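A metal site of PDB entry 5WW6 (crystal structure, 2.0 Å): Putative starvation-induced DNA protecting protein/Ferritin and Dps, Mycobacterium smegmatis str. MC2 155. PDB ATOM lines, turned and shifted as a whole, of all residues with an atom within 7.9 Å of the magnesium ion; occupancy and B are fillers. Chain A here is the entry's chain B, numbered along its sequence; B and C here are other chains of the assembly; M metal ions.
The magnesium ion is bound by the side-chain amide oxygen (OD1) of Asn 48 of chain A, the side-chain amide oxygen (OD1) of Asn 48 of chain B, the side-chain amide oxygen (OD1) of Asn 48 of chain C, the side-chain carboxylate (OD2) of Asp 51 of chain C, the side-chain carboxylate (OD2) of Asp 51 of chain B and the side-chain carboxylate (OD2) of Asp 51 of chain A. The magnesium ion has six donor atoms within binding distance.
N of Asn 48 of chain C lies within hydrogen-bond range of OE1 of Glu 157 of chain B. The guanidinium group (NH1) of Arg 50 of chain B lies within salt-bridge range of the side-chain carboxylate (OD1) of Asp 51 of chain A (2.9 Å). NH1 of Arg 50 of chain C is in salt-bridge range of OD1 of Asp 51 of chain B (2.9 Å). N of Asn 48 of chain B sits at hydrogen-bond distance from OE2 of Glu 157 of chain A. ND2 of Asn 48 of chain C lies within hydrogen-bond range of OE2 of Glu 157 of chain C (2.9 Å). The side-chain amide nitrogen (ND2) of Asn 48 of chain A sits at hydrogen-bond distance from the side-chain carboxylate (OE2) of Glu 157 of chain A, at 2.8 Å. The guanidinium group (NH1) of Arg 50 of chain A lies within salt-bridge range of the side-chain carboxylate (OD1) of Asp 51 of chain C. N of Asn 48 of chain A is in hydrogen-bond range of OE2 of Glu 157 of chain C (2.8 Å).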
ATOM      1  N   SER A  47      20.564  -3.777   0.307  1.00  0.00           N
ATOM      2  CA  SER A  47      20.422  -2.820  -0.784  1.00  0.00           C
ATOM      3  C   SER A  47      21.267  -1.571  -0.565  1.00  0.00           C
ATOM      4  O   SER A  47      21.170  -0.939   0.477  1.00  0.00           O
ATOM      5  CB  SER A  47      18.953  -2.419  -0.943  1.00  0.00           C
ATOM      6  OG  SER A  47      18.805  -1.343  -1.850  1.00  0.00           O
ATOM      7  N   ASN A  48      22.097  -1.247  -1.565  1.00  0.00           N
ATOM      8  CA  ASN A  48      23.036  -0.123  -1.517  1.00  0.00           C
ATOM      9  C   ASN A  48      24.113  -0.245  -0.429  1.00  0.00           C
ATOM     10  O   ASN A  48      24.580   0.754   0.142  1.00  0.00           O
ATOM     11  CB  ASN A  48      22.309   1.224  -1.439  1.00  0.00           C
ATOM     12  CG  ASN A  48      23.157   2.362  -1.946  1.00  0.00           C
ATOM     13  OD1 ASN A  48      24.021   2.164  -2.811  1.00  0.00           O
ATOM     14  ND2 ASN A  48      22.938   3.561  -1.417  1.00  0.00           N
ATOM     15  N   PHE A  49      24.522  -1.494  -0.174  1.00  0.00           N
ATOM     16  CA  PHE A  49      25.635  -1.820   0.713  1.00  0.00           C
ATOM     17  C   PHE A  49      26.859  -0.922   0.507  1.00  0.00           C
ATOM     18  O   PHE A  49      27.364  -0.321   1.459  1.00  0.00           O
ATOM     19  CB  PHE A  49      26.038  -3.297   0.554  1.00  0.00           C
ATOM     20  CG  PHE A  49      27.409  -3.597   1.108  1.00  0.00           C
ATOM     21  CD1 PHE A  49      27.613  -3.695   2.483  1.00  0.00           C
ATOM     22  CD2 PHE A  49      28.504  -3.774   0.243  1.00  0.00           C
ATOM     23  CE1 PHE A  49      28.888  -3.959   3.005  1.00  0.00           C
ATOM     24  CE2 PHE A  49      29.770  -4.025   0.759  1.00  0.00           C
ATOM     25  CZ  PHE A  49      29.961  -4.119   2.130  1.00  0.00           C
ATOM     26  N   ARG A  50      27.334  -0.853  -0.730  1.00  0.00           N
ATOM     27  CA  ARG A  50      28.654  -0.300  -1.003  1.00  0.00           C
ATOM     28  C   ARG A  50      28.734   1.197  -0.643  1.00  0.00           C
ATOM     29  O   ARG A  50      29.672   1.598   0.050  1.00  0.00           O
ATOM     30  CB  ARG A  50      29.065  -0.564  -2.452  1.00  0.00           C
ATOM     31  CG  ARG A  50      30.455  -0.060  -2.783  1.00  0.00           C
ATOM     32  CD  ARG A  50      30.797  -0.396  -4.223  1.00  0.00           C
ATOM     33  NE  ARG A  50      32.141   0.077  -4.577  1.00  0.00           N
ATOM     34  CZ  ARG A  50      32.430   1.294  -5.013  1.00  0.00           C
ATOM     35  NH1 ARG A  50      31.480   2.219  -5.162  1.00  0.00           N
ATOM     36  NH2 ARG A  50      33.696   1.599  -5.302  1.00  0.00           N
ATOM     37  N   ASP A  51      27.750   1.980  -1.090  1.00  0.00           N
ATOM     38  CA  ASP A  51      27.658   3.394  -0.727  1.00  0.00           C
ATOM     39  C   ASP A  51      27.714   3.612   0.773  1.00  0.00           C
ATOM     40  O   ASP A  51      28.420   4.512   1.237  1.00  0.00           O
ATOM     41  CB  ASP A  51      26.372   4.038  -1.277  1.00  0.00           C
ATOM     42  CG  ASP A  51      26.553   4.668  -2.656  1.00  0.00           C
ATOM     43  OD1 ASP A  51      27.628   5.232  -2.956  1.00  0.00           O
ATOM     44  OD2 ASP A  51      25.585   4.613  -3.435  1.00  0.00           O
ATOM     45  N   LEU A  52      26.969   2.799   1.529  1.00  0.00           N
ATOM     46  CA  LEU A  52      26.960   2.927   2.991  1.00  0.00           C
ATOM     47  C   LEU A  52      28.277   2.537   3.623  1.00  0.00           C
ATOM     48  O   LEU A  52      28.796   3.276   4.450  1.00  0.00           O
ATOM     49  CB  LEU A  52      25.813   2.122   3.640  1.00  0.00           C
ATOM     50  CG  LEU A  52      24.527   2.886   3.981  1.00  0.00           C
ATOM     51  CD1 LEU A  52      24.793   4.030   4.964  1.00  0.00           C
ATOM     52  CD2 LEU A  52      23.796   3.364   2.726  1.00  0.00           C
ATOM     53  N   GLU A 157      19.532   8.643   2.200  1.00  0.00           N
ATOM     54  CA  GLU A 157      19.228   7.286   1.707  1.00  0.00           C
ATOM     55  C   GLU A 157      17.810   6.785   2.074  1.00  0.00           C
ATOM     56  O   GLU A 157      17.173   6.107   1.273  1.00  0.00           O
ATOM     57  CB  GLU A 157      20.303   6.301   2.205  1.00  0.00           C
ATOM     58  CG  GLU A 157      20.043   4.811   1.953  1.00  0.00           C
ATOM     59  CD  GLU A 157      20.149   4.377   0.491  1.00  0.00           C
ATOM     60  OE1 GLU A 157      19.566   3.327   0.152  1.00  0.00           O
ATOM     61  OE2 GLU A 157      20.813   5.063  -0.308  1.00  0.00           O
ATOM     62  N   SER B  47      16.499   6.275  -2.116  1.00  0.00           N
ATOM     63  CA  SER B  47      17.263   5.059  -2.408  1.00  0.00           C
ATOM     64  C   SER B  47      18.422   5.315  -3.379  1.00  0.00           C
ATOM     65  O   SER B  47      18.212   5.861  -4.461  1.00  0.00           O
ATOM     66  CB  SER B  47      16.348   3.964  -2.933  1.00  0.00           C
ATOM     67  OG  SER B  47      15.371   3.630  -1.963  1.00  0.00           O
ATOM     68  N   ASN B  48      19.617   4.903  -2.978  1.00  0.00           N
ATOM     69  CA  ASN B  48      20.875   5.123  -3.720  1.00  0.00           C
ATOM     70  C   ASN B  48      21.245   6.612  -3.888  1.00  0.00           C
ATOM     71  O   ASN B  48      21.787   7.032  -4.924  1.00  0.00           O
ATOM     72  CB  ASN B  48      20.889   4.372  -5.081  1.00  0.00           C
ATOM     73  CG  ASN B  48      22.301   4.091  -5.557  1.00  0.00           C
ATOM     74  OD1 ASN B  48      23.225   3.993  -4.750  1.00  0.00           O
ATOM     75  ND2 ASN B  48      22.484   3.979  -6.869  1.00  0.00           N
ATOM     76  N   PHE B  49      20.953   7.402  -2.836  1.00  0.00           N
ATOM     77  CA  PHE B  49      21.297   8.829  -2.794  1.00  0.00           C
ATOM     78  C   PHE B  49      22.765   9.082  -3.158  1.00  0.00           C
ATOM     79  O   PHE B  49      23.049   9.913  -4.003  1.00  0.00           O
ATOM     80  CB  PHE B  49      21.023   9.424  -1.390  1.00  0.00           C
ATOM     81  CG  PHE B  49      21.730  10.741  -1.147  1.00  0.00           C
ATOM     82  CD1 PHE B  49      22.912  10.789  -0.382  1.00  0.00           C
ATOM     83  CD2 PHE B  49      21.227  11.931  -1.692  1.00  0.00           C
ATOM     84  CE1 PHE B  49      23.566  11.993  -0.162  1.00  0.00           C
ATOM     85  CE2 PHE B  49      21.892  13.141  -1.477  1.00  0.00           C
ATOM     86  CZ  PHE B  49      23.068  13.170  -0.709  1.00  0.00           C
ATOM     87  N   ARG B  50      23.683   8.377  -2.499  1.00  0.00           N
ATOM     88  CA  ARG B  50      25.107   8.701  -2.575  1.00  0.00           C
ATOM     89  C   ARG B  50      25.677   8.570  -3.996  1.00  0.00           C
ATOM     90  O   ARG B  50      26.331   9.498  -4.472  1.00  0.00           O
ATOM     91  CB  ARG B  50      25.923   7.882  -1.559  1.00  0.00           C
ATOM     92  CG  ARG B  50      27.394   8.248  -1.501  1.00  0.00           C
ATOM     93  CD  ARG B  50      28.123   7.476  -0.409  1.00  0.00           C
ATOM     94  NE  ARG B  50      29.551   7.788  -0.398  1.00  0.00           N
ATOM     95  CZ  ARG B  50      30.474   7.204  -1.158  1.00  0.00           C
ATOM     96  NH1 ARG B  50      30.158   6.238  -2.022  1.00  0.00           N
ATOM     97  NH2 ARG B  50      31.747   7.585  -1.060  1.00  0.00           N
ATOM     98  N   ASP B  51      25.424   7.440  -4.651  1.00  0.00           N
ATOM     99  CA  ASP B  51      25.844   7.222  -6.047  1.00  0.00           C
ATOM    100  C   ASP B  51      25.397   8.359  -6.964  1.00  0.00           C
ATOM    101  O   ASP B  51      26.184   8.869  -7.760  1.00  0.00           O
ATOM    102  CB  ASP B  51      25.300   5.903  -6.579  1.00  0.00           C
ATOM    103  CG  ASP B  51      26.256   4.747  -6.406  1.00  0.00           C
ATOM    104  OD1 ASP B  51      27.478   4.926  -6.544  1.00  0.00           O
ATOM    105  OD2 ASP B  51      25.767   3.627  -6.116  1.00  0.00           O
ATOM    106  N   LEU B  52      24.127   8.732  -6.842  1.00  0.00           N
ATOM    107  CA  LEU B  52      23.540   9.811  -7.638  1.00  0.00           C
ATOM    108  C   LEU B  52      24.138  11.162  -7.309  1.00  0.00           C
ATOM    109  O   LEU B  52      24.532  11.889  -8.209  1.00  0.00           O
ATOM    110  CB  LEU B  52      22.016   9.836  -7.482  1.00  0.00           C
ATOM    111  CG  LEU B  52      21.190   9.109  -8.560  1.00  0.00           C
ATOM    112  CD1 LEU B  52      21.490   9.668  -9.954  1.00  0.00           C
ATOM    113  CD2 LEU B  52      21.407   7.602  -8.498  1.00  0.00           C
ATOM    114  N   GLU B 157      20.453   3.331 -13.615  1.00  0.00           N
ATOM    115  CA  GLU B 157      19.795   3.213 -12.303  1.00  0.00           C
ATOM    116  C   GLU B 157      18.301   2.831 -12.373  1.00  0.00           C
ATOM    117  O   GLU B 157      17.841   2.019 -11.566  1.00  0.00           O
ATOM    118  CB  GLU B 157      19.974   4.511 -11.496  1.00  0.00           C
ATOM    119  CG  GLU B 157      19.250   4.576 -10.148  1.00  0.00           C
ATOM    120  CD  GLU B 157      19.773   3.590  -9.096  1.00  0.00           C
ATOM    121  OE1 GLU B 157      20.976   3.256  -9.074  1.00  0.00           O
ATOM    122  OE2 GLU B 157      18.953   3.159  -8.260  1.00  0.00           O
ATOM    123  N   SER C  47      18.757  -1.018 -10.208  1.00  0.00           N
ATOM    124  CA  SER C  47      18.935  -0.436  -8.878  1.00  0.00           C
ATOM    125  C   SER C  47      20.366  -0.594  -8.383  1.00  0.00           C
ATOM    126  O   SER C  47      20.890  -1.707  -8.357  1.00  0.00           O
ATOM    127  CB  SER C  47      17.958  -1.084  -7.884  1.00  0.00           C
ATOM    128  OG  SER C  47      18.034  -0.446  -6.614  1.00  0.00           O
ATOM    129  N   ASN C  48      20.979   0.524  -8.012  1.00  0.00           N
ATOM    130  CA  ASN C  48      22.364   0.579  -7.533  1.00  0.00           C
ATOM    131  C   ASN C  48      23.409   0.205  -8.590  1.00  0.00           C
ATOM    132  O   ASN C  48      24.458  -0.383  -8.279  1.00  0.00           O
ATOM    133  CB  ASN C  48      22.571  -0.225  -6.235  1.00  0.00           C
ATOM    134  CG  ASN C  48      23.759   0.268  -5.438  1.00  0.00           C
ATOM    135  OD1 ASN C  48      24.105   1.446  -5.536  1.00  0.00           O
ATOM    136  ND2 ASN C  48      24.391  -0.609  -4.680  1.00  0.00           N
ATOM    137  N   PHE C  49      23.100   0.583  -9.840  1.00  0.00           N
ATOM    138  CA  PHE C  49      23.986   0.365 -10.982  1.00  0.00           C
ATOM    139  C   PHE C  49      25.400   0.871 -10.715  1.00  0.00           C
ATOM    140  O   PHE C  49      26.362   0.157 -10.965  1.00  0.00           O
ATOM    141  CB  PHE C  49      23.436   1.047 -12.263  1.00  0.00           C
ATOM    142  CG  PHE C  49      24.491   1.328 -13.295  1.00  0.00           C
ATOM    143  CD1 PHE C  49      24.924   0.316 -14.154  1.00  0.00           C
ATOM    144  CD2 PHE C  49      25.083   2.587 -13.387  1.00  0.00           C
ATOM    145  CE1 PHE C  49      25.917   0.554 -15.090  1.00  0.00           C
ATOM    146  CE2 PHE C  49      26.083   2.834 -14.315  1.00  0.00           C
ATOM    147  CZ  PHE C  49      26.503   1.826 -15.179  1.00  0.00           C
ATOM    148  N   ARG C  50      25.513   2.108 -10.233  1.00  0.00           N
ATOM    149  CA  ARG C  50      26.817   2.783 -10.152  1.00  0.00           C
ATOM    150  C   ARG C  50      27.782   2.043  -9.228  1.00  0.00           C
ATOM    151  O   ARG C  50      28.909   1.755  -9.634  1.00  0.00           O
ATOM    152  CB  ARG C  50      26.669   4.267  -9.793  1.00  0.00           C
ATOM    153  CG  ARG C  50      27.971   5.044  -9.841  1.00  0.00           C
ATOM    154  CD  ARG C  50      27.784   6.497  -9.487  1.00  0.00           C
ATOM    155  NE  ARG C  50      29.066   7.212  -9.482  1.00  0.00           N
ATOM    156  CZ  ARG C  50      29.877   7.317  -8.437  1.00  0.00           C
ATOM    157  NH1 ARG C  50      29.583   6.738  -7.281  1.00  0.00           N
ATOM    158  NH2 ARG C  50      31.008   8.002  -8.550  1.00  0.00           N
ATOM    159  N   ASP C  51      27.336   1.709  -8.014  1.00  0.00           N
ATOM    160  CA  ASP C  51      28.152   0.945  -7.063  1.00  0.00           C
ATOM    161  C   ASP C  51      28.681  -0.349  -7.655  1.00  0.00           C
ATOM    162  O   ASP C  51      29.866  -0.651  -7.501  1.00  0.00           O
ATOM    163  CB  ASP C  51      27.377   0.627  -5.790  1.00  0.00           C
ATOM    164  CG  ASP C  51      27.560   1.653  -4.693  1.00  0.00           C
ATOM    165  OD1 ASP C  51      28.676   2.197  -4.537  1.00  0.00           O
ATOM    166  OD2 ASP C  51      26.579   1.913  -3.970  1.00  0.00           O
ATOM    167  N   LEU C  52      27.796  -1.090  -8.317  1.00  0.00           N
ATOM    168  CA  LEU C  52      28.166  -2.369  -8.932  1.00  0.00           C
ATOM    169  C   LEU C  52      29.110  -2.220 -10.114  1.00  0.00           C
ATOM    170  O   LEU C  52      30.098  -2.953 -10.199  1.00  0.00           O
ATOM    171  CB  LEU C  52      26.918  -3.194  -9.311  1.00  0.00           C
ATOM    172  CG  LEU C  52      26.369  -4.193  -8.277  1.00  0.00           C
ATOM    173  CD1 LEU C  52      27.440  -5.196  -7.845  1.00  0.00           C
ATOM    174  CD2 LEU C  52      25.752  -3.513  -7.062  1.00  0.00           C
ATOM    175  N   GLU C 157      25.215  -6.742  -1.172  1.00  0.00           N
ATOM    176  CA  GLU C 157      24.120  -6.034  -1.834  1.00  0.00           C
ATOM    177  C   GLU C 157      22.797  -6.819  -1.821  1.00  0.00           C
ATOM    178  O   GLU C 157      21.741  -6.223  -1.651  1.00  0.00           O
ATOM    179  CB  GLU C 157      24.537  -5.710  -3.290  1.00  0.00           C
ATOM    180  CG  GLU C 157      23.432  -5.180  -4.220  1.00  0.00           C
ATOM    181  CD  GLU C 157      22.895  -3.811  -3.822  1.00  0.00           C
ATOM    182  OE1 GLU C 157      21.728  -3.528  -4.163  1.00  0.00           O
ATOM    183  OE2 GLU C 157      23.609  -3.020  -3.187  1.00  0.00           O
HETATM  184 MG    MG M   1      24.871   2.947  -4.406  1.00  0.00          MG
